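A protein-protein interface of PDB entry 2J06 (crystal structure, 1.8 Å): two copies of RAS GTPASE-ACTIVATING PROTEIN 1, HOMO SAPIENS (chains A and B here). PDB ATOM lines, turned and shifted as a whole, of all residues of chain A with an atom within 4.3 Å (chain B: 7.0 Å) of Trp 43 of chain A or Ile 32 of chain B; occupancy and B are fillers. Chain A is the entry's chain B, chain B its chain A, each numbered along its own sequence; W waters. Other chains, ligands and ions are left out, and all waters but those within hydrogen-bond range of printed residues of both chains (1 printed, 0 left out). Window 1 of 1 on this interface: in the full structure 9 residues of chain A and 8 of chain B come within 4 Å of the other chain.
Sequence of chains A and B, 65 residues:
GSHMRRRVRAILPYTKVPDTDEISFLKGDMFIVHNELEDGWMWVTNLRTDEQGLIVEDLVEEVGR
Water W1 lies within hydrogen-bond range of the side-chain carboxylate of Asp 21 of chain A (2.7 Å) and the guanidinium group of Arg 7 of chain B (3.3 Å).
Positions printed for both chains: 33, 34, 35, 42, 43 and 44.
Of the 10 pairs that touch across the chains among the printed residues, none has its exchanged pair printed and touching as well.
Arg 6 of chain B touches Asp 21 of chain A.
CG2 of Thr 45 of chain B touches CD2 of Leu 37 of chain A, at 3.5 Å.
CZ2 of Trp 43 of chain A touches NH1 of Arg 7 of chain B, 3.6 Å away.
Ile 32 of chain B touches Trp 43 of chain A (CD1 to CE3, 3.8 Å).
Leu 47 of chain B touches Trp 43 of chain A.
Met 4 of chain B touches Leu 54 of chain A (O to CD1, 3.4 Å).
O of Arg 5 of chain B touches CD1 of Leu 54 of chain A (3.7 Å).
Printed residues of chain B that touch a printed residue of chain A: Met 4, Arg 5, Arg 6, Arg 7, Ile 32, Thr 45 and Leu 47.
Hydrophobic or aromatic side chains of chain B that line the printed part of chain A: Ile 32 and Leu 47.
The guanidinium group of Arg 5 of chain B lies within hydrogen-bond range of the backbone carbonyl oxygen of Val 33 of chain B.
The guanidinium group (NH2) of Arg 5 of chain B sits at hydrogen-bond distance from the backbone carbonyl oxygen (O) of His 34 of chain B.
The backbone NH of Ile 32 of chain B lies within hydrogen-bond range of the backbone carbonyl oxygen of Thr 45 of chain B, 3.0 Å away.
A ring nitrogen (NE2) of His 34 of chain B is in hydrogen-bond range of the side-chain hydroxyl (OG1) of Thr 45 of chain B (2.6 Å).
The backbone NH (N) of Leu 54 of chain A is in hydrogen-bond range of the backbone carbonyl oxygen (O) of Asp 21 of chain A (2.9 Å).
O of Asn 35 of chain A lies within hydrogen-bond range of N of Trp 43 of chain A (2.9 Å).
The backbone carbonyl oxygen of Arg 5 of chain B lies within hydrogen-bond range of the backbone NH of Asp 21 of chain A (2.6 Å).
OD2 of Asp 21 of chain A sits at hydrogen-bond distance from N of Arg 7 of chain B (2.7 Å).
The backbone carbonyl oxygen of Leu 47 of chain B is in hydrogen-bond range of the side-chain amide nitrogen of Asn 35 of chain A, 2.9 Å away.
Printed residues of chain B within 4 Å of Asn 35 of chain A: Leu 47.
Of the printed residues of chain B, Leu 37 of chain A touches Thr 45 (3.5 Å).
Met 42 of chain A touches none of the printed residues of chain B.
Of the printed residues of chain B, Trp 43 of chain A touches Arg 7, Ile 32 and Leu 47.
Printed residues of chain B within 4 Å of Leu 54 of chain A: Met 4 and Arg 5.
Of the printed residues of chain A, Arg 6 of chain B touches Asp 21 (3.2 Å).
The nearest residue of chain B that does not touch Trp 43 of chain A is Met 30 of chain B (6.5 Å).
The nearest printed residue of chain A that does not touch Ile 32 of chain B is Leu 37 of chain A (4.1 Å).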
ATOM      1  N   ASP A  21      11.952 -27.026 -31.828  1.00  0.00           N
ATOM      2  CA  ASP A  21      10.656 -27.623 -32.047  1.00  0.00           C
ATOM      3  C   ASP A  21       9.614 -26.603 -32.474  1.00  0.00           C
ATOM      4  O   ASP A  21       8.424 -26.735 -32.195  1.00  0.00           O
ATOM      5  CB  ASP A  21      10.240 -28.435 -30.826  1.00  0.00           C
ATOM      6  CG  ASP A  21      10.978 -29.768 -30.763  1.00  0.00           C
ATOM      7  OD1 ASP A  21      10.746 -30.614 -31.656  1.00  0.00           O
ATOM      8  OD2 ASP A  21      11.808 -29.962 -29.854  1.00  0.00           O
ATOM      9  N   VAL A  33      -4.422 -23.838 -29.499  1.00  0.00           N
ATOM     10  CA  VAL A  33      -3.435 -23.603 -28.448  1.00  0.00           C
ATOM     11  C   VAL A  33      -3.564 -24.596 -27.296  1.00  0.00           C
ATOM     12  O   VAL A  33      -4.629 -24.722 -26.686  1.00  0.00           O
ATOM     13  CB  VAL A  33      -3.566 -22.163 -27.899  1.00  0.00           C
ATOM     14  CG1 VAL A  33      -2.454 -21.870 -26.887  1.00  0.00           C
ATOM     15  CG2 VAL A  33      -3.511 -21.168 -29.053  1.00  0.00           C
ATOM     16  N   HIS A  34      -2.476 -25.302 -27.008  1.00  0.00           N
ATOM     17  CA  HIS A  34      -2.456 -26.288 -25.935  1.00  0.00           C
ATOM     18  C   HIS A  34      -1.817 -25.721 -24.670  1.00  0.00           C
ATOM     19  O   HIS A  34      -2.278 -25.986 -23.563  1.00  0.00           O
ATOM     20  CB  HIS A  34      -1.697 -27.533 -26.383  1.00  0.00           C
ATOM     21  CG  HIS A  34      -2.245 -28.158 -27.624  1.00  0.00           C
ATOM     22  ND1 HIS A  34      -3.583 -28.449 -27.777  1.00  0.00           N
ATOM     23  CD2 HIS A  34      -1.641 -28.556 -28.768  1.00  0.00           C
ATOM     24  CE1 HIS A  34      -3.780 -28.999 -28.962  1.00  0.00           C
ATOM     25  NE2 HIS A  34      -2.616 -29.075 -29.584  1.00  0.00           N
ATOM     26  N   ASN A  35      -0.754 -24.940 -24.839  1.00  0.00           N
ATOM     27  CA  ASN A  35      -0.059 -24.329 -23.710  1.00  0.00           C
ATOM     28  C   ASN A  35       0.400 -22.934 -24.081  1.00  0.00           C
ATOM     29  O   ASN A  35       0.831 -22.692 -25.209  1.00  0.00           O
ATOM     30  CB  ASN A  35       1.195 -25.120 -23.318  1.00  0.00           C
ATOM     31  CG  ASN A  35       0.919 -26.577 -23.047  1.00  0.00           C
ATOM     32  OD1 ASN A  35       0.733 -27.367 -23.971  1.00  0.00           O
ATOM     33  ND2 ASN A  35       0.892 -26.946 -21.770  1.00  0.00           N
ATOM     34  N   LEU A  37       3.156 -20.379 -23.047  1.00  0.00           N
ATOM     35  CA  LEU A  37       4.399 -20.301 -22.307  1.00  0.00           C
ATOM     36  C   LEU A  37       4.842 -18.858 -22.089  1.00  0.00           C
ATOM     37  O   LEU A  37       4.185 -17.917 -22.537  1.00  0.00           O
ATOM     38  CB  LEU A  37       5.465 -21.093 -23.062  1.00  0.00           C
ATOM     39  CG  LEU A  37       4.975 -22.503 -23.432  1.00  0.00           C
ATOM     40  CD1 LEU A  37       5.818 -23.091 -24.544  1.00  0.00           C
ATOM     41  CD2 LEU A  37       5.004 -23.388 -22.197  1.00  0.00           C
ATOM     42  N   MET A  42       3.888 -20.378 -27.573  1.00  0.00           N
ATOM     43  CA  MET A  42       2.748 -21.263 -27.394  1.00  0.00           C
ATOM     44  C   MET A  42       3.016 -22.630 -28.003  1.00  0.00           C
ATOM     45  O   MET A  42       3.684 -22.734 -29.034  1.00  0.00           O
ATOM     46  CB  MET A  42       1.497 -20.674 -28.066  1.00  0.00           C
ATOM     47  CG  MET A  42       1.060 -19.325 -27.537  1.00  0.00           C
ATOM     48  SD  MET A  42      -0.458 -18.673 -28.536  1.00  0.00           S
ATOM     49  CE  MET A  42       0.449 -18.276 -30.168  1.00  0.00           C
ATOM     50  N   TRP A  43       2.511 -23.675 -27.347  1.00  0.00           N
ATOM     51  CA  TRP A  43       2.636 -25.033 -27.865  1.00  0.00           C
ATOM     52  C   TRP A  43       1.270 -25.240 -28.514  1.00  0.00           C
ATOM     53  O   TRP A  43       0.242 -25.132 -27.849  1.00  0.00           O
ATOM     54  CB  TRP A  43       2.878 -26.047 -26.740  1.00  0.00           C
ATOM     55  CG  TRP A  43       3.010 -27.444 -27.259  1.00  0.00           C
ATOM     56  CD1 TRP A  43       2.047 -28.415 -27.256  1.00  0.00           C
ATOM     57  CD2 TRP A  43       4.144 -28.008 -27.933  1.00  0.00           C
ATOM     58  NE1 TRP A  43       2.510 -29.543 -27.889  1.00  0.00           N
ATOM     59  CE2 TRP A  43       3.793 -29.323 -28.315  1.00  0.00           C
ATOM     60  CE3 TRP A  43       5.423 -27.530 -28.253  1.00  0.00           C
ATOM     61  CZ2 TRP A  43       4.671 -30.167 -29.002  1.00  0.00           C
ATOM     62  CZ3 TRP A  43       6.298 -28.367 -28.935  1.00  0.00           C
ATOM     63  CH2 TRP A  43       5.916 -29.675 -29.303  1.00  0.00           C
ATOM     64  N   VAL A  44       1.268 -25.520 -29.815  1.00  0.00           N
ATOM     65  CA  VAL A  44       0.033 -25.635 -30.580  1.00  0.00           C
ATOM     66  C   VAL A  44       0.026 -26.786 -31.585  1.00  0.00           C
ATOM     67  O   VAL A  44       1.009 -27.504 -31.739  1.00  0.00           O
ATOM     68  CB  VAL A  44      -0.196 -24.338 -31.425  1.00  0.00           C
ATOM     69  CG1 VAL A  44      -0.116 -23.094 -30.555  1.00  0.00           C
ATOM     70  CG2 VAL A  44       0.858 -24.256 -32.519  1.00  0.00           C
ATOM     71  N   GLN A  52       2.550 -30.579 -34.367  1.00  0.00           N
ATOM     72  CA  GLN A  52       2.525 -29.956 -33.046  1.00  0.00           C
ATOM     73  C   GLN A  52       3.862 -29.245 -32.917  1.00  0.00           C
ATOM     74  O   GLN A  52       4.885 -29.755 -33.376  1.00  0.00           O
ATOM     75  CB  GLN A  52       2.426 -31.000 -31.933  1.00  0.00           C
ATOM     76  CG  GLN A  52       1.071 -31.650 -31.773  1.00  0.00           C
ATOM     77  CD  GLN A  52       1.056 -32.618 -30.609  1.00  0.00           C
ATOM     78  OE1 GLN A  52       1.298 -32.234 -29.463  1.00  0.00           O
ATOM     79  NE2 GLN A  52       0.778 -33.884 -30.896  1.00  0.00           N
ATOM     80  N   GLY A  53       3.863 -28.077 -32.296  1.00  0.00           N
ATOM     81  CA  GLY A  53       5.111 -27.362 -32.139  1.00  0.00           C
ATOM     82  C   GLY A  53       4.921 -25.999 -31.522  1.00  0.00           C
ATOM     83  O   GLY A  53       3.809 -25.613 -31.167  1.00  0.00           O
ATOM     84  N   LEU A  54       6.023 -25.270 -31.396  1.00  0.00           N
ATOM     85  CA  LEU A  54       6.009 -23.933 -30.824  1.00  0.00           C
ATOM     86  C   LEU A  54       5.838 -22.846 -31.883  1.00  0.00           C
ATOM     87  O   LEU A  54       6.392 -22.952 -32.974  1.00  0.00           O
ATOM     88  CB  LEU A  54       7.326 -23.674 -30.089  1.00  0.00           C
ATOM     89  CG  LEU A  54       7.642 -24.484 -28.829  1.00  0.00           C
ATOM     90  CD1 LEU A  54       9.103 -24.311 -28.465  1.00  0.00           C
ATOM     91  CD2 LEU A  54       6.752 -24.018 -27.691  1.00  0.00           C
ATOM     92  N   MET B   4      12.393 -19.622 -28.278  1.00  0.00           N
ATOM     93  CA  MET B   4      12.081 -20.737 -29.214  1.00  0.00           C
ATOM     94  C   MET B   4      12.508 -22.111 -28.620  1.00  0.00           C
ATOM     95  O   MET B   4      11.949 -22.561 -27.627  1.00  0.00           O
ATOM     96  CB  MET B   4      12.795 -20.465 -30.532  1.00  0.00           C
ATOM     97  CG  MET B   4      14.281 -20.251 -30.359  1.00  0.00           C
ATOM     98  SD  MET B   4      15.187 -20.340 -32.037  1.00  0.00           S
ATOM     99  CE  MET B   4      16.790 -19.426 -31.495  1.00  0.00           C
ATOM    100  N   ARG B   5      13.487 -22.771 -29.235  1.00  0.00           N
ATOM    101  CA  ARG B   5      14.039 -24.060 -28.799  1.00  0.00           C
ATOM    102  C   ARG B   5      13.294 -25.409 -28.862  1.00  0.00           C
ATOM    103  O   ARG B   5      12.370 -25.607 -29.646  1.00  0.00           O
ATOM    104  CB  ARG B   5      14.670 -23.917 -27.422  1.00  0.00           C
ATOM    105  CG  ARG B   5      16.192 -23.825 -27.535  1.00  0.00           C
ATOM    106  CD  ARG B   5      16.919 -24.220 -26.277  1.00  0.00           C
ATOM    107  NE  ARG B   5      17.443 -23.062 -25.556  1.00  0.00           N
ATOM    108  CZ  ARG B   5      16.709 -22.045 -25.117  1.00  0.00           C
ATOM    109  NH1 ARG B   5      15.399 -22.025 -25.323  1.00  0.00           N
ATOM    110  NH2 ARG B   5      17.297 -21.052 -24.464  1.00  0.00           N
ATOM    111  N   ARG B   6      13.743 -26.339 -28.017  1.00  0.00           N
ATOM    112  CA  ARG B   6      13.280 -27.724 -28.041  1.00  0.00           C
ATOM    113  C   ARG B   6      12.524 -28.375 -26.889  1.00  0.00           C
ATOM    114  O   ARG B   6      12.486 -27.896 -25.755  1.00  0.00           O
ATOM    115  CB  ARG B   6      14.484 -28.614 -28.347  1.00  0.00           C
ATOM    116  CG  ARG B   6      15.456 -28.725 -27.187  1.00  0.00           C
ATOM    117  CD  ARG B   6      16.645 -29.615 -27.546  1.00  0.00           C
ATOM    118  NE  ARG B   6      17.360 -30.083 -26.360  1.00  0.00           N
ATOM    119  CZ  ARG B   6      17.981 -29.293 -25.491  1.00  0.00           C
ATOM    120  NH1 ARG B   6      17.986 -27.979 -25.665  1.00  0.00           N
ATOM    121  NH2 ARG B   6      18.591 -29.818 -24.437  1.00  0.00           N
ATOM    122  N   ARG B   7      11.972 -29.536 -27.229  1.00  0.00           N
ATOM    123  CA  ARG B   7      11.189 -30.374 -26.335  1.00  0.00           C
ATOM    124  C   ARG B   7      11.977 -31.626 -25.945  1.00  0.00           C
ATOM    125  O   ARG B   7      12.671 -32.211 -26.778  1.00  0.00           O
ATOM    126  CB  ARG B   7       9.901 -30.795 -27.052  1.00  0.00           C
ATOM    127  CG  ARG B   7       9.082 -31.845 -26.322  1.00  0.00           C
ATOM    128  CD  ARG B   7       7.789 -32.199 -27.071  1.00  0.00           C
ATOM    129  NE  ARG B   7       8.047 -32.677 -28.427  1.00  0.00           N
ATOM    130  CZ  ARG B   7       7.158 -33.312 -29.189  1.00  0.00           C
ATOM    131  NH1 ARG B   7       5.938 -33.555 -28.733  1.00  0.00           N
ATOM    132  NH2 ARG B   7       7.490 -33.700 -30.412  1.00  0.00           N
ATOM    133  N   VAL B   8      11.886 -32.020 -24.675  1.00  0.00           N
ATOM    134  CA  VAL B   8      12.547 -33.232 -24.186  1.00  0.00           C
ATOM    135  C   VAL B   8      11.491 -34.055 -23.443  1.00  0.00           C
ATOM    136  O   VAL B   8      10.441 -33.527 -23.083  1.00  0.00           O
ATOM    137  CB  VAL B   8      13.742 -32.927 -23.232  1.00  0.00           C
ATOM    138  CG1 VAL B   8      14.831 -32.149 -23.986  1.00  0.00           C
ATOM    139  CG2 VAL B   8      13.270 -32.143 -22.008  1.00  0.00           C
ATOM    140  N   MET B  30       6.395 -34.312 -21.278  1.00  0.00           N
ATOM    141  CA  MET B  30       7.128 -33.516 -22.264  1.00  0.00           C
ATOM    142  C   MET B  30       7.418 -32.141 -21.662  1.00  0.00           C
ATOM    143  O   MET B  30       6.571 -31.562 -20.973  1.00  0.00           O
ATOM    144  CB  MET B  30       6.303 -33.342 -23.544  1.00  0.00           C
ATOM    145  CG  MET B  30       6.027 -34.632 -24.279  1.00  0.00           C
ATOM    146  SD  MET B  30       7.619 -35.316 -25.104  1.00  0.00           S
ATOM    147  CE  MET B  30       6.809 -35.991 -26.724  1.00  0.00           C
ATOM    148  N   PHE B  31       8.613 -31.627 -21.932  1.00  0.00           N
ATOM    149  CA  PHE B  31       9.036 -30.323 -21.418  1.00  0.00           C
ATOM    150  C   PHE B  31       9.589 -29.458 -22.538  1.00  0.00           C
ATOM    151  O   PHE B  31      10.162 -29.972 -23.495  1.00  0.00           O
ATOM    152  CB  PHE B  31      10.187 -30.464 -20.417  1.00  0.00           C
ATOM    153  CG  PHE B  31       9.941 -31.440 -19.308  1.00  0.00           C
ATOM    154  CD1 PHE B  31       9.446 -31.008 -18.085  1.00  0.00           C
ATOM    155  CD2 PHE B  31      10.270 -32.785 -19.467  1.00  0.00           C
ATOM    156  CE1 PHE B  31       9.286 -31.896 -17.023  1.00  0.00           C
ATOM    157  CE2 PHE B  31      10.113 -33.684 -18.408  1.00  0.00           C
ATOM    158  CZ  PHE B  31       9.621 -33.235 -17.185  1.00  0.00           C
ATOM    159  N   ILE B  32       9.446 -28.146 -22.391  1.00  0.00           N
ATOM    160  CA  ILE B  32      10.024 -27.206 -23.345  1.00  0.00           C
ATOM    161  C   ILE B  32      11.196 -26.637 -22.562  1.00  0.00           C
ATOM    162  O   ILE B  32      11.028 -26.154 -21.440  1.00  0.00           O
ATOM    163  CB  ILE B  32       9.054 -26.062 -23.715  1.00  0.00           C
ATOM    164  CG1 ILE B  32       7.876 -26.625 -24.520  1.00  0.00           C
ATOM    165  CG2 ILE B  32       9.809 -24.955 -24.477  1.00  0.00           C
ATOM    166  CD1 ILE B  32       8.290 -27.404 -25.744  1.00  0.00           C
ATOM    167  N   VAL B  33      12.386 -26.715 -23.136  1.00  0.00           N
ATOM    168  CA  VAL B  33      13.571 -26.227 -22.451  1.00  0.00           C
ATOM    169  C   VAL B  33      13.795 -24.733 -22.652  1.00  0.00           C
ATOM    170  O   VAL B  33      13.828 -24.249 -23.783  1.00  0.00           O
ATOM    171  CB  VAL B  33      14.815 -27.000 -22.916  1.00  0.00           C
ATOM    172  CG1 VAL B  33      16.047 -26.513 -22.159  1.00  0.00           C
ATOM    173  CG2 VAL B  33      14.593 -28.492 -22.701  1.00  0.00           C
ATOM    174  N   HIS B  34      13.935 -24.008 -21.546  1.00  0.00           N
ATOM    175  CA  HIS B  34      14.172 -22.568 -21.599  1.00  0.00           C
ATOM    176  C   HIS B  34      15.658 -22.269 -21.417  1.00  0.00           C
ATOM    177  O   HIS B  34      16.226 -21.467 -22.159  1.00  0.00           O
ATOM    178  CB  HIS B  34      13.365 -21.857 -20.514  1.00  0.00           C
ATOM    179  CG  HIS B  34      11.896 -22.137 -20.581  1.00  0.00           C
ATOM    180  ND1 HIS B  34      11.169 -22.010 -21.744  1.00  0.00           N
ATOM    181  CD2 HIS B  34      11.017 -22.525 -19.628  1.00  0.00           C
ATOM    182  CE1 HIS B  34       9.904 -22.306 -21.505  1.00  0.00           C
ATOM    183  NE2 HIS B  34       9.785 -22.622 -20.229  1.00  0.00           N
ATOM    184  N   ASN B  35      16.279 -22.911 -20.430  1.00  0.00           N
ATOM    185  CA  ASN B  35      17.706 -22.722 -20.164  1.00  0.00           C
ATOM    186  C   ASN B  35      18.390 -24.031 -19.807  1.00  0.00           C
ATOM    187  O   ASN B  35      17.839 -24.851 -19.075  1.00  0.00           O
ATOM    188  CB  ASN B  35      17.952 -21.778 -18.982  1.00  0.00           C
ATOM    189  CG  ASN B  35      17.230 -20.462 -19.110  1.00  0.00           C
ATOM    190  OD1 ASN B  35      16.051 -20.355 -18.781  1.00  0.00           O
ATOM    191  ND2 ASN B  35      17.938 -19.442 -19.584  1.00  0.00           N
ATOM    192  N   MET B  42      18.220 -27.859 -15.779  1.00  0.00           N
ATOM    193  CA  MET B  42      17.623 -27.005 -16.790  1.00  0.00           C
ATOM    194  C   MET B  42      16.333 -26.376 -16.279  1.00  0.00           C
ATOM    195  O   MET B  42      15.650 -26.941 -15.424  1.00  0.00           O
ATOM    196  CB  MET B  42      17.375 -27.801 -18.088  1.00  0.00           C
ATOM    197  CG  MET B  42      16.979 -29.261 -17.889  1.00  0.00           C
ATOM    198  SD  MET B  42      17.097 -30.356 -19.511  1.00  0.00           S
ATOM    199  CE  MET B  42      15.235 -30.304 -20.022  1.00  0.00           C
ATOM    200  N   TRP B  43      16.031 -25.181 -16.780  1.00  0.00           N
ATOM    201  CA  TRP B  43      14.818 -24.467 -16.412  1.00  0.00           C
ATOM    202  C   TRP B  43      13.881 -24.791 -17.566  1.00  0.00           C
ATOM    203  O   TRP B  43      14.198 -24.521 -18.723  1.00  0.00           O
ATOM    204  CB  TRP B  43      15.085 -22.956 -16.310  1.00  0.00           C
ATOM    205  CG  TRP B  43      13.902 -22.180 -15.794  1.00  0.00           C
ATOM    206  CD1 TRP B  43      12.984 -21.495 -16.536  1.00  0.00           C
ATOM    207  CD2 TRP B  43      13.472 -22.078 -14.430  1.00  0.00           C
ATOM    208  NE1 TRP B  43      12.006 -20.974 -15.720  1.00  0.00           N
ATOM    209  CE2 TRP B  43      12.280 -21.317 -14.424  1.00  0.00           C
ATOM    210  CE3 TRP B  43      13.975 -22.555 -13.215  1.00  0.00           C
ATOM    211  CZ2 TRP B  43      11.582 -21.027 -13.247  1.00  0.00           C
ATOM    212  CZ3 TRP B  43      13.282 -22.267 -12.046  1.00  0.00           C
ATOM    213  CH2 TRP B  43      12.099 -21.511 -12.070  1.00  0.00           C
ATOM    214  N   VAL B  44      12.741 -25.391 -17.248  1.00  0.00           N
ATOM    215  CA  VAL B  44      11.803 -25.827 -18.275  1.00  0.00           C
ATOM    216  C   VAL B  44      10.356 -25.629 -17.866  1.00  0.00           C
ATOM    217  O   VAL B  44      10.068 -25.208 -16.753  1.00  0.00           O
ATOM    218  CB  VAL B  44      11.958 -27.348 -18.512  1.00  0.00           C
ATOM    219  CG1 VAL B  44      13.421 -27.708 -18.802  1.00  0.00           C
ATOM    220  CG2 VAL B  44      11.485 -28.100 -17.262  1.00  0.00           C
ATOM    221  N   THR B  45       9.452 -25.958 -18.786  1.00  0.00           N
ATOM    222  CA  THR B  45       8.020 -25.932 -18.514  1.00  0.00           C
ATOM    223  C   THR B  45       7.500 -27.332 -18.846  1.00  0.00           C
ATOM    224  O   THR B  45       7.754 -27.852 -19.936  1.00  0.00           O
ATOM    225  CB  THR B  45       7.256 -24.931 -19.395  1.00  0.00           C
ATOM    226  OG1 THR B  45       7.634 -23.595 -19.046  1.00  0.00           O
ATOM    227  CG2 THR B  45       5.751 -25.089 -19.184  1.00  0.00           C
ATOM    228  N   ASN B  46       6.787 -27.937 -17.902  1.00  0.00           N
ATOM    229  CA  ASN B  46       6.200 -29.264 -18.100  1.00  0.00           C
ATOM    230  C   ASN B  46       4.887 -29.016 -18.847  1.00  0.00           C
ATOM    231  O   ASN B  46       4.015 -28.316 -18.345  1.00  0.00           O
ATOM    232  CB  ASN B  46       5.915 -29.922 -16.744  1.00  0.00           C
ATOM    233  CG  ASN B  46       5.370 -31.345 -16.874  1.00  0.00           C
ATOM    234  OD1 ASN B  46       4.517 -31.616 -17.708  1.00  0.00           O
ATOM    235  ND2 ASN B  46       5.860 -32.251 -16.032  1.00  0.00           N
ATOM    236  N   LEU B  47       4.753 -29.574 -20.046  1.00  0.00           N
ATOM    237  CA  LEU B  47       3.550 -29.363 -20.844  1.00  0.00           C
ATOM    238  C   LEU B  47       2.295 -30.040 -20.295  1.00  0.00           C
ATOM    239  O   LEU B  47       1.182 -29.651 -20.636  1.00  0.00           O
ATOM    240  CB  LEU B  47       3.792 -29.813 -22.294  1.00  0.00           C
ATOM    241  CG  LEU B  47       4.862 -29.024 -23.055  1.00  0.00           C
ATOM    242  CD1 LEU B  47       5.022 -29.584 -24.465  1.00  0.00           C
ATOM    243  CD2 LEU B  47       4.465 -27.555 -23.113  1.00  0.00           C
HETATM  244  O   HOH W   1      10.756 -33.067 -30.496  1.00  0.00           O
